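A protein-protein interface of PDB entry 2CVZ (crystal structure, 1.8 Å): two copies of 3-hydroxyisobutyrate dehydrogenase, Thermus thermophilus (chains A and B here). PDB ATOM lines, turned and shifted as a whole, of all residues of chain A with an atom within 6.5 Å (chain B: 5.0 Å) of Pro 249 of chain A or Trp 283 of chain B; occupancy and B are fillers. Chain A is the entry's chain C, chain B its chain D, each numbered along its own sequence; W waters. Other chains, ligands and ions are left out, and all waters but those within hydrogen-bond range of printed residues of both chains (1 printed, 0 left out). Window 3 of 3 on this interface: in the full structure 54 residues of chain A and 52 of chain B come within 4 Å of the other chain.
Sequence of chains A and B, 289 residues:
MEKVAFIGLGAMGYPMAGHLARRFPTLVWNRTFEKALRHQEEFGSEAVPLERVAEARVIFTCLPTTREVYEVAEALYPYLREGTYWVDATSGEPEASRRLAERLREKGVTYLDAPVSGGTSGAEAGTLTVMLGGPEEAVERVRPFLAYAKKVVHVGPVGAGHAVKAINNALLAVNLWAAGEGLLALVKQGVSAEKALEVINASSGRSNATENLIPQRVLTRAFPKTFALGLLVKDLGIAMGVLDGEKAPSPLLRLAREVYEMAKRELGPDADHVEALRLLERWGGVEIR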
ATOM      1  N   GLU A 246     -29.215  -2.503  24.352  1.00  0.00           N
ATOM      2  CA  GLU A 246     -28.784  -1.972  23.063  1.00  0.00           C
ATOM      3  C   GLU A 246     -29.707  -2.454  21.948  1.00  0.00           C
ATOM      4  O   GLU A 246     -29.860  -1.786  20.923  1.00  0.00           O
ATOM      5  CB  GLU A 246     -27.345  -2.430  22.785  1.00  0.00           C
ATOM      6  CG  GLU A 246     -26.838  -2.186  21.367  1.00  0.00           C
ATOM      7  CD  GLU A 246     -26.847  -0.721  20.970  1.00  0.00           C
ATOM      8  OE1 GLU A 246     -26.668   0.143  21.854  1.00  0.00           O
ATOM      9  OE2 GLU A 246     -27.017  -0.432  19.765  1.00  0.00           O
ATOM     10  N   LYS A 247     -30.317  -3.616  22.168  1.00  0.00           N
ATOM     11  CA  LYS A 247     -31.218  -4.237  21.203  1.00  0.00           C
ATOM     12  C   LYS A 247     -30.549  -4.530  19.868  1.00  0.00           C
ATOM     13  O   LYS A 247     -31.152  -4.363  18.805  1.00  0.00           O
ATOM     14  CB  LYS A 247     -32.476  -3.380  20.996  1.00  0.00           C
ATOM     15  CG  LYS A 247     -33.382  -3.360  22.222  1.00  0.00           C
ATOM     16  CD  LYS A 247     -34.693  -2.633  21.971  1.00  0.00           C
ATOM     17  CE  LYS A 247     -35.531  -2.581  23.243  1.00  0.00           C
ATOM     18  NZ  LYS A 247     -36.821  -1.866  23.034  1.00  0.00           N
ATOM     19  N   ALA A 248     -29.290  -4.959  19.925  1.00  0.00           N
ATOM     20  CA  ALA A 248     -28.576  -5.329  18.711  1.00  0.00           C
ATOM     21  C   ALA A 248     -29.247  -6.637  18.300  1.00  0.00           C
ATOM     22  O   ALA A 248     -29.730  -7.374  19.157  1.00  0.00           O
ATOM     23  CB  ALA A 248     -27.106  -5.564  19.008  1.00  0.00           C
ATOM     24  N   PRO A 249     -29.288  -6.943  16.991  1.00  0.00           N
ATOM     25  CA  PRO A 249     -29.922  -8.174  16.501  1.00  0.00           C
ATOM     26  C   PRO A 249     -29.438  -9.421  17.237  1.00  0.00           C
ATOM     27  O   PRO A 249     -28.265  -9.780  17.147  1.00  0.00           O
ATOM     28  CB  PRO A 249     -29.544  -8.189  15.021  1.00  0.00           C
ATOM     29  CG  PRO A 249     -29.436  -6.727  14.690  1.00  0.00           C
ATOM     30  CD  PRO A 249     -28.677  -6.195  15.879  1.00  0.00           C
ATOM     31  N   SER A 250     -30.351 -10.077  17.951  1.00  0.00           N
ATOM     32  CA  SER A 250     -30.027 -11.272  18.730  1.00  0.00           C
ATOM     33  C   SER A 250     -31.089 -12.359  18.533  1.00  0.00           C
ATOM     34  O   SER A 250     -31.724 -12.810  19.491  1.00  0.00           O
ATOM     35  CB  SER A 250     -29.947 -10.907  20.212  1.00  0.00           C
ATOM     36  OG  SER A 250     -29.107  -9.781  20.417  1.00  0.00           O
ATOM     37  N   PRO A 251     -31.272 -12.816  17.288  1.00  0.00           N
ATOM     38  CA  PRO A 251     -32.269 -13.848  16.985  1.00  0.00           C
ATOM     39  C   PRO A 251     -32.201 -15.157  17.776  1.00  0.00           C
ATOM     40  O   PRO A 251     -33.228 -15.647  18.255  1.00  0.00           O
ATOM     41  CB  PRO A 251     -32.094 -14.063  15.479  1.00  0.00           C
ATOM     42  CG  PRO A 251     -30.638 -13.766  15.267  1.00  0.00           C
ATOM     43  CD  PRO A 251     -30.449 -12.522  16.102  1.00  0.00           C
ATOM     44  N   TRP B 177     -22.376 -18.477  17.708  1.00  0.00           N
ATOM     45  CA  TRP B 177     -23.204 -17.315  17.411  1.00  0.00           C
ATOM     46  C   TRP B 177     -23.944 -16.793  18.640  1.00  0.00           C
ATOM     47  O   TRP B 177     -24.000 -15.582  18.864  1.00  0.00           O
ATOM     48  CB  TRP B 177     -24.204 -17.639  16.294  1.00  0.00           C
ATOM     49  CG  TRP B 177     -25.021 -16.455  15.876  1.00  0.00           C
ATOM     50  CD1 TRP B 177     -26.139 -15.962  16.494  1.00  0.00           C
ATOM     51  CD2 TRP B 177     -24.749 -15.577  14.781  1.00  0.00           C
ATOM     52  NE1 TRP B 177     -26.576 -14.829  15.848  1.00  0.00           N
ATOM     53  CE2 TRP B 177     -25.740 -14.570  14.794  1.00  0.00           C
ATOM     54  CE3 TRP B 177     -23.758 -15.541  13.788  1.00  0.00           C
ATOM     55  CZ2 TRP B 177     -25.771 -13.536  13.852  1.00  0.00           C
ATOM     56  CZ3 TRP B 177     -23.789 -14.511  12.851  1.00  0.00           C
ATOM     57  CH2 TRP B 177     -24.789 -13.523  12.892  1.00  0.00           C
ATOM     58  N   GLU B 181     -23.836 -13.031  20.409  1.00  0.00           N
ATOM     59  CA  GLU B 181     -24.958 -12.155  20.750  1.00  0.00           C
ATOM     60  C   GLU B 181     -24.875 -11.760  22.222  1.00  0.00           C
ATOM     61  O   GLU B 181     -25.071 -10.595  22.584  1.00  0.00           O
ATOM     62  CB  GLU B 181     -26.302 -12.864  20.519  1.00  0.00           C
ATOM     63  CG  GLU B 181     -26.615 -13.252  19.077  1.00  0.00           C
ATOM     64  CD  GLU B 181     -27.997 -13.892  18.931  1.00  0.00           C
ATOM     65  OE1 GLU B 181     -28.392 -14.225  17.794  1.00  0.00           O
ATOM     66  OE2 GLU B 181     -28.695 -14.060  19.958  1.00  0.00           O
ATOM     67  N   MET B 262     -26.163 -15.227   6.355  1.00  0.00           N
ATOM     68  CA  MET B 262     -26.089 -13.768   6.354  1.00  0.00           C
ATOM     69  C   MET B 262     -24.628 -13.344   6.454  1.00  0.00           C
ATOM     70  O   MET B 262     -24.163 -12.484   5.702  1.00  0.00           O
ATOM     71  CB  MET B 262     -26.853 -13.181   7.540  1.00  0.00           C
ATOM     72  CG  MET B 262     -28.332 -13.488   7.552  1.00  0.00           C
ATOM     73  SD  MET B 262     -29.160 -12.683   9.093  1.00  0.00           S
ATOM     74  CE  MET B 262     -30.972 -13.328   8.820  1.00  0.00           C
ATOM     75  N   LEU B 279     -20.004  -9.683  11.956  1.00  0.00           N
ATOM     76  CA  LEU B 279     -21.285  -9.121  11.539  1.00  0.00           C
ATOM     77  C   LEU B 279     -22.012  -8.584  12.768  1.00  0.00           C
ATOM     78  O   LEU B 279     -22.618  -7.514  12.721  1.00  0.00           O
ATOM     79  CB  LEU B 279     -22.140 -10.174  10.821  1.00  0.00           C
ATOM     80  CG  LEU B 279     -23.488  -9.671  10.278  1.00  0.00           C
ATOM     81  CD1 LEU B 279     -23.272  -8.420   9.421  1.00  0.00           C
ATOM     82  CD2 LEU B 279     -24.162 -10.769   9.466  1.00  0.00           C
ATOM     83  N   LEU B 280     -21.941  -9.318  13.875  1.00  0.00           N
ATOM     84  CA  LEU B 280     -22.584  -8.872  15.109  1.00  0.00           C
ATOM     85  C   LEU B 280     -21.891  -7.611  15.628  1.00  0.00           C
ATOM     86  O   LEU B 280     -22.535  -6.716  16.181  1.00  0.00           O
ATOM     87  CB  LEU B 280     -22.532  -9.977  16.168  1.00  0.00           C
ATOM     88  CG  LEU B 280     -23.425 -11.187  15.874  1.00  0.00           C
ATOM     89  CD1 LEU B 280     -23.154 -12.303  16.865  1.00  0.00           C
ATOM     90  CD2 LEU B 280     -24.885 -10.762  15.929  1.00  0.00           C
ATOM     91  N   GLU B 281     -20.576  -7.549  15.450  1.00  0.00           N
ATOM     92  CA  GLU B 281     -19.799  -6.391  15.889  1.00  0.00           C
ATOM     93  C   GLU B 281     -20.204  -5.175  15.065  1.00  0.00           C
ATOM     94  O   GLU B 281     -20.325  -4.066  15.592  1.00  0.00           O
ATOM     95  CB  GLU B 281     -18.303  -6.662  15.717  1.00  0.00           C
ATOM     96  CG  GLU B 281     -17.727  -7.595  16.769  1.00  0.00           C
ATOM     97  CD  GLU B 281     -16.262  -7.912  16.543  1.00  0.00           C
ATOM     98  OE1 GLU B 281     -15.596  -8.323  17.514  1.00  0.00           O
ATOM     99  OE2 GLU B 281     -15.778  -7.761  15.400  1.00  0.00           O
ATOM    100  N   ARG B 282     -20.403  -5.388  13.769  1.00  0.00           N
ATOM    101  CA  ARG B 282     -20.809  -4.311  12.877  1.00  0.00           C
ATOM    102  C   ARG B 282     -22.137  -3.720  13.339  1.00  0.00           C
ATOM    103  O   ARG B 282     -22.264  -2.506  13.504  1.00  0.00           O
ATOM    104  CB  ARG B 282     -20.971  -4.822  11.445  1.00  0.00           C
ATOM    105  CG  ARG B 282     -21.492  -3.752  10.491  1.00  0.00           C
ATOM    106  CD  ARG B 282     -22.130  -4.348   9.245  1.00  0.00           C
ATOM    107  NE  ARG B 282     -21.176  -5.081   8.421  1.00  0.00           N
ATOM    108  CZ  ARG B 282     -21.478  -5.618   7.243  1.00  0.00           C
ATOM    109  NH1 ARG B 282     -22.707  -5.499   6.759  1.00  0.00           N
ATOM    110  NH2 ARG B 282     -20.553  -6.267   6.544  1.00  0.00           N
ATOM    111  N   TRP B 283     -23.128  -4.586  13.544  1.00  0.00           N
ATOM    112  CA  TRP B 283     -24.443  -4.132  13.979  1.00  0.00           C
ATOM    113  C   TRP B 283     -24.400  -3.464  15.344  1.00  0.00           C
ATOM    114  O   TRP B 283     -24.997  -2.406  15.543  1.00  0.00           O
ATOM    115  CB  TRP B 283     -25.436  -5.299  14.017  1.00  0.00           C
ATOM    116  CG  TRP B 283     -25.756  -5.869  12.672  1.00  0.00           C
ATOM    117  CD1 TRP B 283     -25.744  -5.208  11.479  1.00  0.00           C
ATOM    118  CD2 TRP B 283     -26.184  -7.205  12.387  1.00  0.00           C
ATOM    119  NE1 TRP B 283     -26.138  -6.047  10.467  1.00  0.00           N
ATOM    120  CE2 TRP B 283     -26.415  -7.281  10.996  1.00  0.00           C
ATOM    121  CE3 TRP B 283     -26.397  -8.347  13.173  1.00  0.00           C
ATOM    122  CZ2 TRP B 283     -26.849  -8.455  10.370  1.00  0.00           C
ATOM    123  CZ3 TRP B 283     -26.829  -9.515  12.551  1.00  0.00           C
ATOM    124  CH2 TRP B 283     -27.050  -9.559  11.162  1.00  0.00           C
ATOM    125  N   GLY B 284     -23.690  -4.081  16.283  1.00  0.00           N
ATOM    126  CA  GLY B 284     -23.604  -3.528  17.621  1.00  0.00           C
ATOM    127  C   GLY B 284     -22.807  -2.243  17.734  1.00  0.00           C
ATOM    128  O   GLY B 284     -22.974  -1.490  18.693  1.00  0.00           O
ATOM    129  N   GLY B 285     -21.937  -1.991  16.763  1.00  0.00           N
ATOM    130  CA  GLY B 285     -21.126  -0.786  16.791  1.00  0.00           C
ATOM    131  C   GLY B 285     -20.013  -0.862  17.820  1.00  0.00           C
ATOM    132  O   GLY B 285     -19.559   0.160  18.334  1.00  0.00           O
HETATM  133  O   HOH W   1     -26.808  -8.650  21.608  1.00  0.00           O
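No position is printed for both chains.
Water W1 lies within hydrogen-bond range of the backbone carbonyl oxygen of Glu 181 of chain B (2.8 Å) and the side-chain hydroxyl of Ser 250 of chain A (2.8 Å).
Hydrophobic or aromatic side chains of chain A that line the printed part of chain B: Pro 249 and Pro 251.
Hydrophobic or aromatic side chains of chain B within 4 Å of the printed part of chain A: Leu 280 and Trp 283.
Among the printed residues, no Asp or Glu carboxylate lies within 4 Å of a Lys or Arg side-chain nitrogen of the other chain.
The backbone carbonyl oxygen (O) of Ala 248 of chain A is in hydrogen-bond range of the side-chain hydroxyl (OG) of Ser 250 of chain A (2.8 Å).
NE1 of Trp 177 of chain B sits at hydrogen-bond distance from OE1 of Glu 181 of chain B (2.7 Å).
N of Pro 251 of chain A sits close to OE1 of Glu 181 of chain B (3.2 Å).
The side-chain carboxylate of Glu 181 of chain B sits close to the backbone carbonyl oxygen of Ser 250 of chain A (3.3 Å).
O of Pro 249 of chain A touches CD2 of Leu 280 of chain B, 3.7 Å away.
Pro 249 of chain A touches Trp 283 of chain B.
Pro 249 of chain A touches just these residues of chain B: Leu 280 and Trp 283.
Trp 283 of chain B touches just one residue of chain A: Pro 249.
Of the printed residues of chain B, Pro 251 of chain A touches Glu 181 (3.2 Å).
Printed residues of chain A within 4 Å of Leu 280 of chain B: Pro 249 (3.7 Å).
Of the printed residues of chain A, Glu 181 of chain B touches Ser 250 and Pro 251.
Of the printed residues of chain B, Ser 250 of chain A touches Glu 181 (3.3 Å).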
